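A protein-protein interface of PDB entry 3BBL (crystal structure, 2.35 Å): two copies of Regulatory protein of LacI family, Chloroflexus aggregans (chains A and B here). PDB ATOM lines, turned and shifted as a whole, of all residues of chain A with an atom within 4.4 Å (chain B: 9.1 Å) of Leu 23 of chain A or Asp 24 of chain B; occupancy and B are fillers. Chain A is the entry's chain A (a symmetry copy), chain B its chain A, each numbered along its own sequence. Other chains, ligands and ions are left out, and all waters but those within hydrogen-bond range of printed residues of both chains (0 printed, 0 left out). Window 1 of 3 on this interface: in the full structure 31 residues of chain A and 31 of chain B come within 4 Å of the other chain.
NE1 of Trp 11 of chain B lies within hydrogen-bond range of OG of Ser 28 of chain A, 2.9 Å away. OG1 of Thr 14 of chain B is in hydrogen-bond range of OD2 of Asp 24 of chain A, 3.1 Å away. The side-chain hydroxyl of Thr 14 of chain A lies within hydrogen-bond range of the side-chain carboxylate of Asp 24 of chain B (3.1 Å). OG of Ser 28 of chain B is in hydrogen-bond range of NE1 of Trp 11 of chain A, 2.9 Å away.
O of Asp 24 of chain B lies within hydrogen-bond range of OG of Ser 28 of chain B. OG of Ser 28 of chain A sits at hydrogen-bond distance from O of Asp 24 of chain A (2.7 Å).
Among the printed residues, pairs that only touch across the chains: Trp 11 of chain A with Asp 24 of chain B, Trp 11 of chain A with Leu 27 of chain B, His 21 of chain A with Asp 24 of chain B, His 21 of chain A with Pro 227 of chain B, Leu 23 of chain A with Asp 24 of chain B, Asp 24 of chain A with Trp 11 of chain B, Asp 24 of chain A with His 21 of chain B, Asp 24 of chain A with Leu 23 of chain B, Leu 27 of chain A with Trp 11 of chain B and Leu 27 of chain A with Leu 27 of chain B.
Printed residues of chain B within 4 Å of Asp 24 of chain A: Trp 11 (3.6 Å), Thr 14 (3.1 Å), His 21 (3.8 Å) and Leu 23 (3.5 Å). Of the printed residues of chain B, Leu 27 of chain A touches Trp 11 (3.9 Å) and Leu 27 (3.5 Å). Of the printed residues of chain A, Thr 14 of chain B touches Asp 24. Of the printed residues of chain A, Leu 23 of chain B touches Asp 24 (3.5 Å). Of chain A, only Trp 11 (3.6 Å), Thr 14 (3.1 Å), His 21 (3.8 Å) and Leu 23 (3.5 Å) come within 4 Å of Asp 24 of chain B. The nearest residue of chain B that does not touch Leu 23 of chain A is Leu 23 of chain B (4.2 Å). The nearest printed residue of chain A that does not touch Asp 24 of chain B is Asp 24 of chain A (6.2 Å). The nearest printed residue of chain A that does not touch Leu 23 of chain B is Leu 23 of chain A (4.2 Å).
Of the 10 printed residues of chain A, 7 touch a printed residue of chain B. Hydrophobic or aromatic side chains of chain A within 4 Å of the printed part of chain B: Trp 11, His 21, Leu 23 and Leu 27. Among the printed residues, no Asp or Glu carboxylate lies within 4 Å of a Lys or Arg side-chain nitrogen of the other chain.
Trp 11 of chain A touches Asp 24 of chain B, and with the chains exchanged Asp 24 of chain A touches Trp 11 of chain B. Trp 11 of chain A touches Leu 27 of chain B, and with the chains exchanged Leu 27 of chain A touches Trp 11 of chain B. His 21 of chain A touches Asp 24 of chain B, and with the chains exchanged Asp 24 of chain A touches His 21 of chain B. Leu 27 of chain A touches its own counterpart, Leu 27 of chain B. Positions printed for both chains: 11, 14, 21, 22, 23, 24, 25, 26, 27 and 28. Of the 14 pairs that touch across the chains among the printed residues, 13 have their exchanged pair printed and touching as well.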
ATOM      1  N   TRP A  11     -16.438  -1.724 -13.196  1.00  0.00           N
ATOM      2  CA  TRP A  11     -15.109  -1.298 -13.612  1.00  0.00           C
ATOM      3  C   TRP A  11     -15.186  -0.216 -14.669  1.00  0.00           C
ATOM      4  O   TRP A  11     -16.126  -0.175 -15.465  1.00  0.00           O
ATOM      5  CB  TRP A  11     -14.297  -2.498 -14.123  1.00  0.00           C
ATOM      6  CG  TRP A  11     -14.934  -3.246 -15.246  1.00  0.00           C
ATOM      7  CD1 TRP A  11     -14.688  -3.092 -16.581  1.00  0.00           C
ATOM      8  CD2 TRP A  11     -15.894  -4.302 -15.134  1.00  0.00           C
ATOM      9  NE1 TRP A  11     -15.428  -4.000 -17.309  1.00  0.00           N
ATOM     10  CE2 TRP A  11     -16.170  -4.756 -16.446  1.00  0.00           C
ATOM     11  CE3 TRP A  11     -16.534  -4.921 -14.054  1.00  0.00           C
ATOM     12  CZ2 TRP A  11     -17.073  -5.793 -16.701  1.00  0.00           C
ATOM     13  CZ3 TRP A  11     -17.431  -5.953 -14.311  1.00  0.00           C
ATOM     14  CH2 TRP A  11     -17.686  -6.383 -15.624  1.00  0.00           C
ATOM     15  N   THR A  14     -12.377   0.369 -20.341  1.00  0.00           N
ATOM     16  CA  THR A  14     -10.996   0.252 -20.796  1.00  0.00           C
ATOM     17  C   THR A  14     -10.799   1.075 -22.063  1.00  0.00           C
ATOM     18  O   THR A  14     -11.513   0.890 -23.049  1.00  0.00           O
ATOM     19  CB  THR A  14     -10.625  -1.204 -21.123  1.00  0.00           C
ATOM     20  OG1 THR A  14     -10.963  -2.049 -20.015  1.00  0.00           O
ATOM     21  CG2 THR A  14      -9.135  -1.317 -21.390  1.00  0.00           C
ATOM     22  N   HIS A  21      -5.137  -5.508 -19.416  1.00  0.00           N
ATOM     23  CA  HIS A  21      -6.532  -5.706 -19.032  1.00  0.00           C
ATOM     24  C   HIS A  21      -6.567  -6.659 -17.842  1.00  0.00           C
ATOM     25  O   HIS A  21      -6.665  -7.878 -18.009  1.00  0.00           O
ATOM     26  CB  HIS A  21      -7.326  -6.305 -20.196  1.00  0.00           C
ATOM     27  CG  HIS A  21      -7.354  -5.438 -21.414  1.00  0.00           C
ATOM     28  ND1 HIS A  21      -8.520  -4.906 -21.922  1.00  0.00           N
ATOM     29  CD2 HIS A  21      -6.358  -4.995 -22.217  1.00  0.00           C
ATOM     30  CE1 HIS A  21      -8.240  -4.171 -22.983  1.00  0.00           C
ATOM     31  NE2 HIS A  21      -6.935  -4.206 -23.185  1.00  0.00           N
ATOM     32  N   ILE A  22      -6.468  -6.098 -16.641  1.00  0.00           N
ATOM     33  CA  ILE A  22      -6.489  -6.902 -15.431  1.00  0.00           C
ATOM     34  C   ILE A  22      -7.913  -7.224 -14.979  1.00  0.00           C
ATOM     35  O   ILE A  22      -8.118  -7.731 -13.880  1.00  0.00           O
ATOM     36  CB  ILE A  22      -5.750  -6.196 -14.273  1.00  0.00           C
ATOM     37  CG1 ILE A  22      -6.437  -4.876 -13.938  1.00  0.00           C
ATOM     38  CG2 ILE A  22      -4.286  -5.975 -14.649  1.00  0.00           C
ATOM     39  CD1 ILE A  22      -5.902  -4.221 -12.690  1.00  0.00           C
ATOM     40  N   LEU A  23      -8.895  -6.919 -15.819  1.00  0.00           N
ATOM     41  CA  LEU A  23     -10.275  -7.218 -15.477  1.00  0.00           C
ATOM     42  C   LEU A  23     -10.380  -8.723 -15.322  1.00  0.00           C
ATOM     43  O   LEU A  23     -10.974  -9.225 -14.374  1.00  0.00           O
ATOM     44  CB  LEU A  23     -11.227  -6.775 -16.588  1.00  0.00           C
ATOM     45  CG  LEU A  23     -12.649  -7.328 -16.419  1.00  0.00           C
ATOM     46  CD1 LEU A  23     -13.355  -6.596 -15.280  1.00  0.00           C
ATOM     47  CD2 LEU A  23     -13.419  -7.172 -17.709  1.00  0.00           C
ATOM     48  N   ASP A  24      -9.783  -9.428 -16.274  1.00  0.00           N
ATOM     49  CA  ASP A  24      -9.796 -10.877 -16.284  1.00  0.00           C
ATOM     50  C   ASP A  24      -9.167 -11.487 -15.040  1.00  0.00           C
ATOM     51  O   ASP A  24      -9.736 -12.398 -14.453  1.00  0.00           O
ATOM     52  CB  ASP A  24      -9.084 -11.396 -17.529  1.00  0.00           C
ATOM     53  CG  ASP A  24      -9.001 -12.906 -17.561  1.00  0.00           C
ATOM     54  OD1 ASP A  24     -10.061 -13.561 -17.655  1.00  0.00           O
ATOM     55  OD2 ASP A  24      -7.874 -13.438 -17.483  1.00  0.00           O
ATOM     56  N   GLN A  25      -8.003 -10.989 -14.633  1.00  0.00           N
ATOM     57  CA  GLN A  25      -7.335 -11.523 -13.446  1.00  0.00           C
ATOM     58  C   GLN A  25      -8.127 -11.229 -12.172  1.00  0.00           C
ATOM     59  O   GLN A  25      -8.359 -12.110 -11.347  1.00  0.00           O
ATOM     60  CB  GLN A  25      -5.936 -10.925 -13.283  1.00  0.00           C
ATOM     61  CG  GLN A  25      -4.923 -11.327 -14.328  1.00  0.00           C
ATOM     62  CD  GLN A  25      -3.569 -10.661 -14.102  1.00  0.00           C
ATOM     63  OE1 GLN A  25      -3.464  -9.432 -14.084  1.00  0.00           O
ATOM     64  NE2 GLN A  25      -2.531 -11.472 -13.932  1.00  0.00           N
ATOM     65  N   PHE A  26      -8.531  -9.972 -12.030  1.00  0.00           N
ATOM     66  CA  PHE A  26      -9.270  -9.508 -10.867  1.00  0.00           C
ATOM     67  C   PHE A  26     -10.668 -10.116 -10.710  1.00  0.00           C
ATOM     68  O   PHE A  26     -10.986 -10.693  -9.668  1.00  0.00           O
ATOM     69  CB  PHE A  26      -9.377  -7.987 -10.921  1.00  0.00           C
ATOM     70  CG  PHE A  26      -9.742  -7.359  -9.618  1.00  0.00           C
ATOM     71  CD1 PHE A  26      -8.884  -7.451  -8.527  1.00  0.00           C
ATOM     72  CD2 PHE A  26     -10.939  -6.667  -9.476  1.00  0.00           C
ATOM     73  CE1 PHE A  26      -9.215  -6.861  -7.301  1.00  0.00           C
ATOM     74  CE2 PHE A  26     -11.282  -6.071  -8.262  1.00  0.00           C
ATOM     75  CZ  PHE A  26     -10.411  -6.172  -7.168  1.00  0.00           C
ATOM     76  N   LEU A  27     -11.496  -9.983 -11.744  1.00  0.00           N
ATOM     77  CA  LEU A  27     -12.852 -10.506 -11.688  1.00  0.00           C
ATOM     78  C   LEU A  27     -12.906 -12.031 -11.635  1.00  0.00           C
ATOM     79  O   LEU A  27     -13.678 -12.601 -10.856  1.00  0.00           O
ATOM     80  CB  LEU A  27     -13.676  -9.986 -12.868  1.00  0.00           C
ATOM     81  CG  LEU A  27     -15.157 -10.382 -12.891  1.00  0.00           C
ATOM     82  CD1 LEU A  27     -15.855  -9.947 -11.602  1.00  0.00           C
ATOM     83  CD2 LEU A  27     -15.824  -9.750 -14.094  1.00  0.00           C
ATOM     84  N   SER A  28     -12.094 -12.698 -12.448  1.00  0.00           N
ATOM     85  CA  SER A  28     -12.080 -14.159 -12.436  1.00  0.00           C
ATOM     86  C   SER A  28     -11.764 -14.631 -11.027  1.00  0.00           C
ATOM     87  O   SER A  28     -12.434 -15.505 -10.484  1.00  0.00           O
ATOM     88  CB  SER A  28     -11.030 -14.709 -13.404  1.00  0.00           C
ATOM     89  OG  SER A  28     -11.392 -14.447 -14.745  1.00  0.00           O
ATOM     90  N   TYR B   9     -23.517 -16.200 -16.728  1.00  0.00           N
ATOM     91  CA  TYR B   9     -22.417 -16.281 -17.677  1.00  0.00           C
ATOM     92  C   TYR B   9     -21.158 -16.810 -17.001  1.00  0.00           C
ATOM     93  O   TYR B   9     -20.953 -16.620 -15.807  1.00  0.00           O
ATOM     94  CB  TYR B   9     -22.123 -14.905 -18.300  1.00  0.00           C
ATOM     95  CG  TYR B   9     -21.003 -14.942 -19.321  1.00  0.00           C
ATOM     96  CD1 TYR B   9     -21.090 -15.765 -20.442  1.00  0.00           C
ATOM     97  CD2 TYR B   9     -19.827 -14.210 -19.132  1.00  0.00           C
ATOM     98  CE1 TYR B   9     -20.043 -15.871 -21.343  1.00  0.00           C
ATOM     99  CE2 TYR B   9     -18.767 -14.310 -20.031  1.00  0.00           C
ATOM    100  CZ  TYR B   9     -18.877 -15.148 -21.134  1.00  0.00           C
ATOM    101  OH  TYR B   9     -17.818 -15.303 -22.010  1.00  0.00           O
ATOM    102  N   TRP B  11     -16.796 -17.962 -18.111  1.00  0.00           N
ATOM    103  CA  TRP B  11     -15.782 -17.997 -19.155  1.00  0.00           C
ATOM    104  C   TRP B  11     -14.629 -18.899 -18.769  1.00  0.00           C
ATOM    105  O   TRP B  11     -14.306 -19.043 -17.588  1.00  0.00           O
ATOM    106  CB  TRP B  11     -15.281 -16.579 -19.463  1.00  0.00           C
ATOM    107  CG  TRP B  11     -14.730 -15.845 -18.287  1.00  0.00           C
ATOM    108  CD1 TRP B  11     -13.418 -15.739 -17.923  1.00  0.00           C
ATOM    109  CD2 TRP B  11     -15.473 -15.071 -17.337  1.00  0.00           C
ATOM    110  NE1 TRP B  11     -13.296 -14.934 -16.811  1.00  0.00           N
ATOM    111  CE2 TRP B  11     -14.539 -14.508 -16.435  1.00  0.00           C
ATOM    112  CE3 TRP B  11     -16.833 -14.787 -17.171  1.00  0.00           C
ATOM    113  CZ2 TRP B  11     -14.930 -13.687 -15.373  1.00  0.00           C
ATOM    114  CZ3 TRP B  11     -17.220 -13.968 -16.114  1.00  0.00           C
ATOM    115  CH2 TRP B  11     -16.270 -13.422 -15.233  1.00  0.00           C
ATOM    116  N   THR B  14      -8.343 -17.969 -18.768  1.00  0.00           N
ATOM    117  CA  THR B  14      -7.399 -17.465 -19.760  1.00  0.00           C
ATOM    118  C   THR B  14      -6.009 -18.024 -19.483  1.00  0.00           C
ATOM    119  O   THR B  14      -5.479 -17.869 -18.383  1.00  0.00           O
ATOM    120  CB  THR B  14      -7.302 -15.931 -19.727  1.00  0.00           C
ATOM    121  OG1 THR B  14      -8.614 -15.361 -19.804  1.00  0.00           O
ATOM    122  CG2 THR B  14      -6.478 -15.433 -20.902  1.00  0.00           C
ATOM    123  N   ASN B  20      -4.499 -11.882 -26.223  1.00  0.00           N
ATOM    124  CA  ASN B  20      -5.841 -11.319 -26.307  1.00  0.00           C
ATOM    125  C   ASN B  20      -6.765 -11.724 -25.154  1.00  0.00           C
ATOM    126  O   ASN B  20      -6.746 -12.870 -24.687  1.00  0.00           O
ATOM    127  CB  ASN B  20      -6.466 -11.691 -27.655  1.00  0.00           C
ATOM    128  CG  ASN B  20      -7.705 -10.878 -27.958  1.00  0.00           C
ATOM    129  OD1 ASN B  20      -7.869  -9.765 -27.436  1.00  0.00           O
ATOM    130  ND2 ASN B  20      -8.579 -11.412 -28.810  1.00  0.00           N
ATOM    131  N   HIS B  21      -7.555 -10.756 -24.697  1.00  0.00           N
ATOM    132  CA  HIS B  21      -8.514 -10.949 -23.612  1.00  0.00           C
ATOM    133  C   HIS B  21      -9.800 -10.217 -23.980  1.00  0.00           C
ATOM    134  O   HIS B  21      -9.980  -9.044 -23.640  1.00  0.00           O
ATOM    135  CB  HIS B  21      -7.958 -10.390 -22.300  1.00  0.00           C
ATOM    136  CG  HIS B  21      -6.692 -11.051 -21.853  1.00  0.00           C
ATOM    137  ND1 HIS B  21      -6.602 -11.762 -20.676  1.00  0.00           N
ATOM    138  CD2 HIS B  21      -5.472 -11.125 -22.433  1.00  0.00           C
ATOM    139  CE1 HIS B  21      -5.379 -12.247 -20.550  1.00  0.00           C
ATOM    140  NE2 HIS B  21      -4.673 -11.877 -21.604  1.00  0.00           N
ATOM    141  N   ILE B  22     -10.685 -10.908 -24.691  1.00  0.00           N
ATOM    142  CA  ILE B  22     -11.948 -10.319 -25.101  1.00  0.00           C
ATOM    143  C   ILE B  22     -13.008 -10.410 -24.005  1.00  0.00           C
ATOM    144  O   ILE B  22     -14.179 -10.132 -24.245  1.00  0.00           O
ATOM    145  CB  ILE B  22     -12.496 -10.992 -26.378  1.00  0.00           C
ATOM    146  CG1 ILE B  22     -12.763 -12.472 -26.117  1.00  0.00           C
ATOM    147  CG2 ILE B  22     -11.510 -10.805 -27.528  1.00  0.00           C
ATOM    148  CD1 ILE B  22     -13.487 -13.158 -27.247  1.00  0.00           C
ATOM    149  N   LEU B  23     -12.602 -10.811 -22.806  1.00  0.00           N
ATOM    150  CA  LEU B  23     -13.542 -10.899 -21.701  1.00  0.00           C
ATOM    151  C   LEU B  23     -14.075  -9.500 -21.458  1.00  0.00           C
ATOM    152  O   LEU B  23     -15.273  -9.295 -21.290  1.00  0.00           O
ATOM    153  CB  LEU B  23     -12.852 -11.384 -20.426  1.00  0.00           C
ATOM    154  CG  LEU B  23     -13.716 -11.212 -19.170  1.00  0.00           C
ATOM    155  CD1 LEU B  23     -14.837 -12.249 -19.170  1.00  0.00           C
ATOM    156  CD2 LEU B  23     -12.862 -11.355 -17.932  1.00  0.00           C
ATOM    157  N   ASP B  24     -13.157  -8.542 -21.450  1.00  0.00           N
ATOM    158  CA  ASP B  24     -13.494  -7.152 -21.221  1.00  0.00           C
ATOM    159  C   ASP B  24     -14.474  -6.600 -22.248  1.00  0.00           C
ATOM    160  O   ASP B  24     -15.439  -5.945 -21.878  1.00  0.00           O
ATOM    161  CB  ASP B  24     -12.226  -6.303 -21.210  1.00  0.00           C
ATOM    162  CG  ASP B  24     -12.521  -4.828 -21.048  1.00  0.00           C
ATOM    163  OD1 ASP B  24     -13.028  -4.434 -19.976  1.00  0.00           O
ATOM    164  OD2 ASP B  24     -12.250  -4.063 -21.997  1.00  0.00           O
ATOM    165  N   GLN B  25     -14.235  -6.865 -23.530  1.00  0.00           N
ATOM    166  CA  GLN B  25     -15.131  -6.369 -24.574  1.00  0.00           C
ATOM    167  C   GLN B  25     -16.509  -7.024 -24.496  1.00  0.00           C
ATOM    168  O   GLN B  25     -17.538  -6.353 -24.534  1.00  0.00           O
ATOM    169  CB  GLN B  25     -14.557  -6.637 -25.966  1.00  0.00           C
ATOM    170  CG  GLN B  25     -13.313  -5.860 -26.328  1.00  0.00           C
ATOM    171  CD  GLN B  25     -12.798  -6.214 -27.719  1.00  0.00           C
ATOM    172  OE1 GLN B  25     -12.481  -7.373 -28.000  1.00  0.00           O
ATOM    173  NE2 GLN B  25     -12.711  -5.217 -28.591  1.00  0.00           N
ATOM    174  N   PHE B  26     -16.505  -8.347 -24.388  1.00  0.00           N
ATOM    175  CA  PHE B  26     -17.724  -9.137 -24.330  1.00  0.00           C
ATOM    176  C   PHE B  26     -18.581  -8.905 -23.081  1.00  0.00           C
ATOM    177  O   PHE B  26     -19.765  -8.578 -23.187  1.00  0.00           O
ATOM    178  CB  PHE B  26     -17.362 -10.617 -24.435  1.00  0.00           C
ATOM    179  CG  PHE B  26     -18.512 -11.497 -24.794  1.00  0.00           C
ATOM    180  CD1 PHE B  26     -19.141 -11.366 -26.027  1.00  0.00           C
ATOM    181  CD2 PHE B  26     -18.968 -12.464 -23.905  1.00  0.00           C
ATOM    182  CE1 PHE B  26     -20.217 -12.191 -26.377  1.00  0.00           C
ATOM    183  CE2 PHE B  26     -20.038 -13.294 -24.239  1.00  0.00           C
ATOM    184  CZ  PHE B  26     -20.665 -13.154 -25.485  1.00  0.00           C
ATOM    185  N   LEU B  27     -17.982  -9.076 -21.906  1.00  0.00           N
ATOM    186  CA  LEU B  27     -18.713  -8.901 -20.661  1.00  0.00           C
ATOM    187  C   LEU B  27     -19.141  -7.456 -20.414  1.00  0.00           C
ATOM    188  O   LEU B  27     -20.278  -7.205 -20.002  1.00  0.00           O
ATOM    189  CB  LEU B  27     -17.891  -9.421 -19.480  1.00  0.00           C
ATOM    190  CG  LEU B  27     -18.575  -9.386 -18.106  1.00  0.00           C
ATOM    191  CD1 LEU B  27     -19.895 -10.157 -18.138  1.00  0.00           C
ATOM    192  CD2 LEU B  27     -17.642  -9.974 -17.069  1.00  0.00           C
ATOM    193  N   SER B  28     -18.246  -6.505 -20.664  1.00  0.00           N
ATOM    194  CA  SER B  28     -18.595  -5.100 -20.466  1.00  0.00           C
ATOM    195  C   SER B  28     -19.815  -4.778 -21.311  1.00  0.00           C
ATOM    196  O   SER B  28     -20.775  -4.176 -20.838  1.00  0.00           O
ATOM    197  CB  SER B  28     -17.439  -4.182 -20.873  1.00  0.00           C
ATOM    198  OG  SER B  28     -16.347  -4.323 -19.988  1.00  0.00           O
ATOM    199  N   SER B  29     -19.767  -5.198 -22.566  1.00  0.00           N
ATOM    200  CA  SER B  29     -20.859  -4.971 -23.491  1.00  0.00           C
ATOM    201  C   SER B  29     -22.161  -5.611 -23.009  1.00  0.00           C
ATOM    202  O   SER B  29     -23.219  -4.991 -23.084  1.00  0.00           O
ATOM    203  CB  SER B  29     -20.490  -5.512 -24.871  1.00  0.00           C
ATOM    204  OG  SER B  29     -21.566  -5.374 -25.773  1.00  0.00           O
ATOM    205  N   MET B  30     -22.093  -6.848 -22.519  1.00  0.00           N
ATOM    206  CA  MET B  30     -23.297  -7.513 -22.032  1.00  0.00           C
ATOM    207  C   MET B  30     -23.851  -6.800 -20.799  1.00  0.00           C
ATOM    208  O   MET B  30     -25.053  -6.552 -20.706  1.00  0.00           O
ATOM    209  CB  MET B  30     -23.033  -8.992 -21.714  1.00  0.00           C
ATOM    210  CG  MET B  30     -22.807  -9.804 -22.959  1.00  0.00           C
ATOM    211  SD  MET B  30     -23.123 -11.752 -22.738  1.00  0.00           S
ATOM    212  CE  MET B  30     -21.742 -12.055 -21.413  1.00  0.00           C
ATOM    213  N   VAL B  31     -22.971  -6.452 -19.866  1.00  0.00           N
ATOM    214  CA  VAL B  31     -23.393  -5.774 -18.653  1.00  0.00           C
ATOM    215  C   VAL B  31     -24.127  -4.473 -18.941  1.00  0.00           C
ATOM    216  O   VAL B  31     -25.145  -4.184 -18.322  1.00  0.00           O
ATOM    217  CB  VAL B  31     -22.194  -5.482 -17.737  1.00  0.00           C
ATOM    218  CG1 VAL B  31     -22.611  -4.554 -16.598  1.00  0.00           C
ATOM    219  CG2 VAL B  31     -21.652  -6.787 -17.177  1.00  0.00           C
ATOM    220  N   ARG B  32     -23.619  -3.693 -19.884  1.00  0.00           N
ATOM    221  CA  ARG B  32     -24.250  -2.421 -20.226  1.00  0.00           C
ATOM    222  C   ARG B  32     -25.554  -2.597 -20.985  1.00  0.00           C
ATOM    223  O   ARG B  32     -26.487  -1.825 -20.810  1.00  0.00           O
ATOM    224  CB  ARG B  32     -23.293  -1.561 -21.048  1.00  0.00           C
ATOM    225  CG  ARG B  32     -22.081  -1.130 -20.265  1.00  0.00           C
ATOM    226  CD  ARG B  32     -21.332  -0.020 -20.967  1.00  0.00           C
ATOM    227  NE  ARG B  32     -20.799   0.900 -19.973  1.00  0.00           N
ATOM    228  CZ  ARG B  32     -21.535   1.779 -19.298  1.00  0.00           C
ATOM    229  NH1 ARG B  32     -22.838   1.876 -19.514  1.00  0.00           N
ATOM    230  NH2 ARG B  32     -20.971   2.535 -18.372  1.00  0.00           N
ATOM    231  N   PRO B 227      -5.200  -6.153 -28.341  1.00  0.00           N
ATOM    232  CA  PRO B 227      -4.685  -4.817 -28.048  1.00  0.00           C
ATOM    233  C   PRO B 227      -3.167  -4.828 -28.074  1.00  0.00           C
ATOM    234  O   PRO B 227      -2.545  -5.783 -27.609  1.00  0.00           O
ATOM    235  CB  PRO B 227      -5.247  -4.535 -26.660  1.00  0.00           C
ATOM    236  CG  PRO B 227      -5.284  -5.891 -26.038  1.00  0.00           C
ATOM    237  CD  PRO B 227      -5.850  -6.737 -27.157  1.00  0.00           C
ATOM    238  N   ILE B 243     -16.610  -8.188 -31.092  1.00  0.00           N
ATOM    239  CA  ILE B 243     -16.934  -8.794 -29.812  1.00  0.00           C
ATOM    240  C   ILE B 243     -17.976  -8.019 -29.014  1.00  0.00           C
ATOM    241  O   ILE B 243     -18.850  -8.624 -28.394  1.00  0.00           O
ATOM    242  CB  ILE B 243     -15.653  -8.979 -28.957  1.00  0.00           C
ATOM    243  CG1 ILE B 243     -14.625  -9.793 -29.753  1.00  0.00           C
ATOM    244  CG2 ILE B 243     -15.981  -9.673 -27.630  1.00  0.00           C
ATOM    245  CD1 ILE B 243     -15.175 -11.102 -30.314  1.00  0.00           C
ATOM    246  N   ALA B 244     -17.893  -6.693 -29.029  1.00  0.00           N
ATOM    247  CA  ALA B 244     -18.864  -5.891 -28.295  1.00  0.00           C
ATOM    248  C   ALA B 244     -20.256  -6.105 -28.887  1.00  0.00           C
ATOM    249  O   ALA B 244     -21.214  -6.356 -28.158  1.00  0.00           O
ATOM    250  CB  ALA B 244     -18.487  -4.411 -28.345  1.00  0.00           C
ATOM    251  N   GLY B 247     -21.689  -9.323 -28.001  1.00  0.00           N
ATOM    252  CA  GLY B 247     -22.152  -9.334 -26.629  1.00  0.00           C
ATOM    253  C   GLY B 247     -23.549  -8.758 -26.561  1.00  0.00           C
ATOM    254  O   GLY B 247     -24.441  -9.331 -25.954  1.00  0.00           O
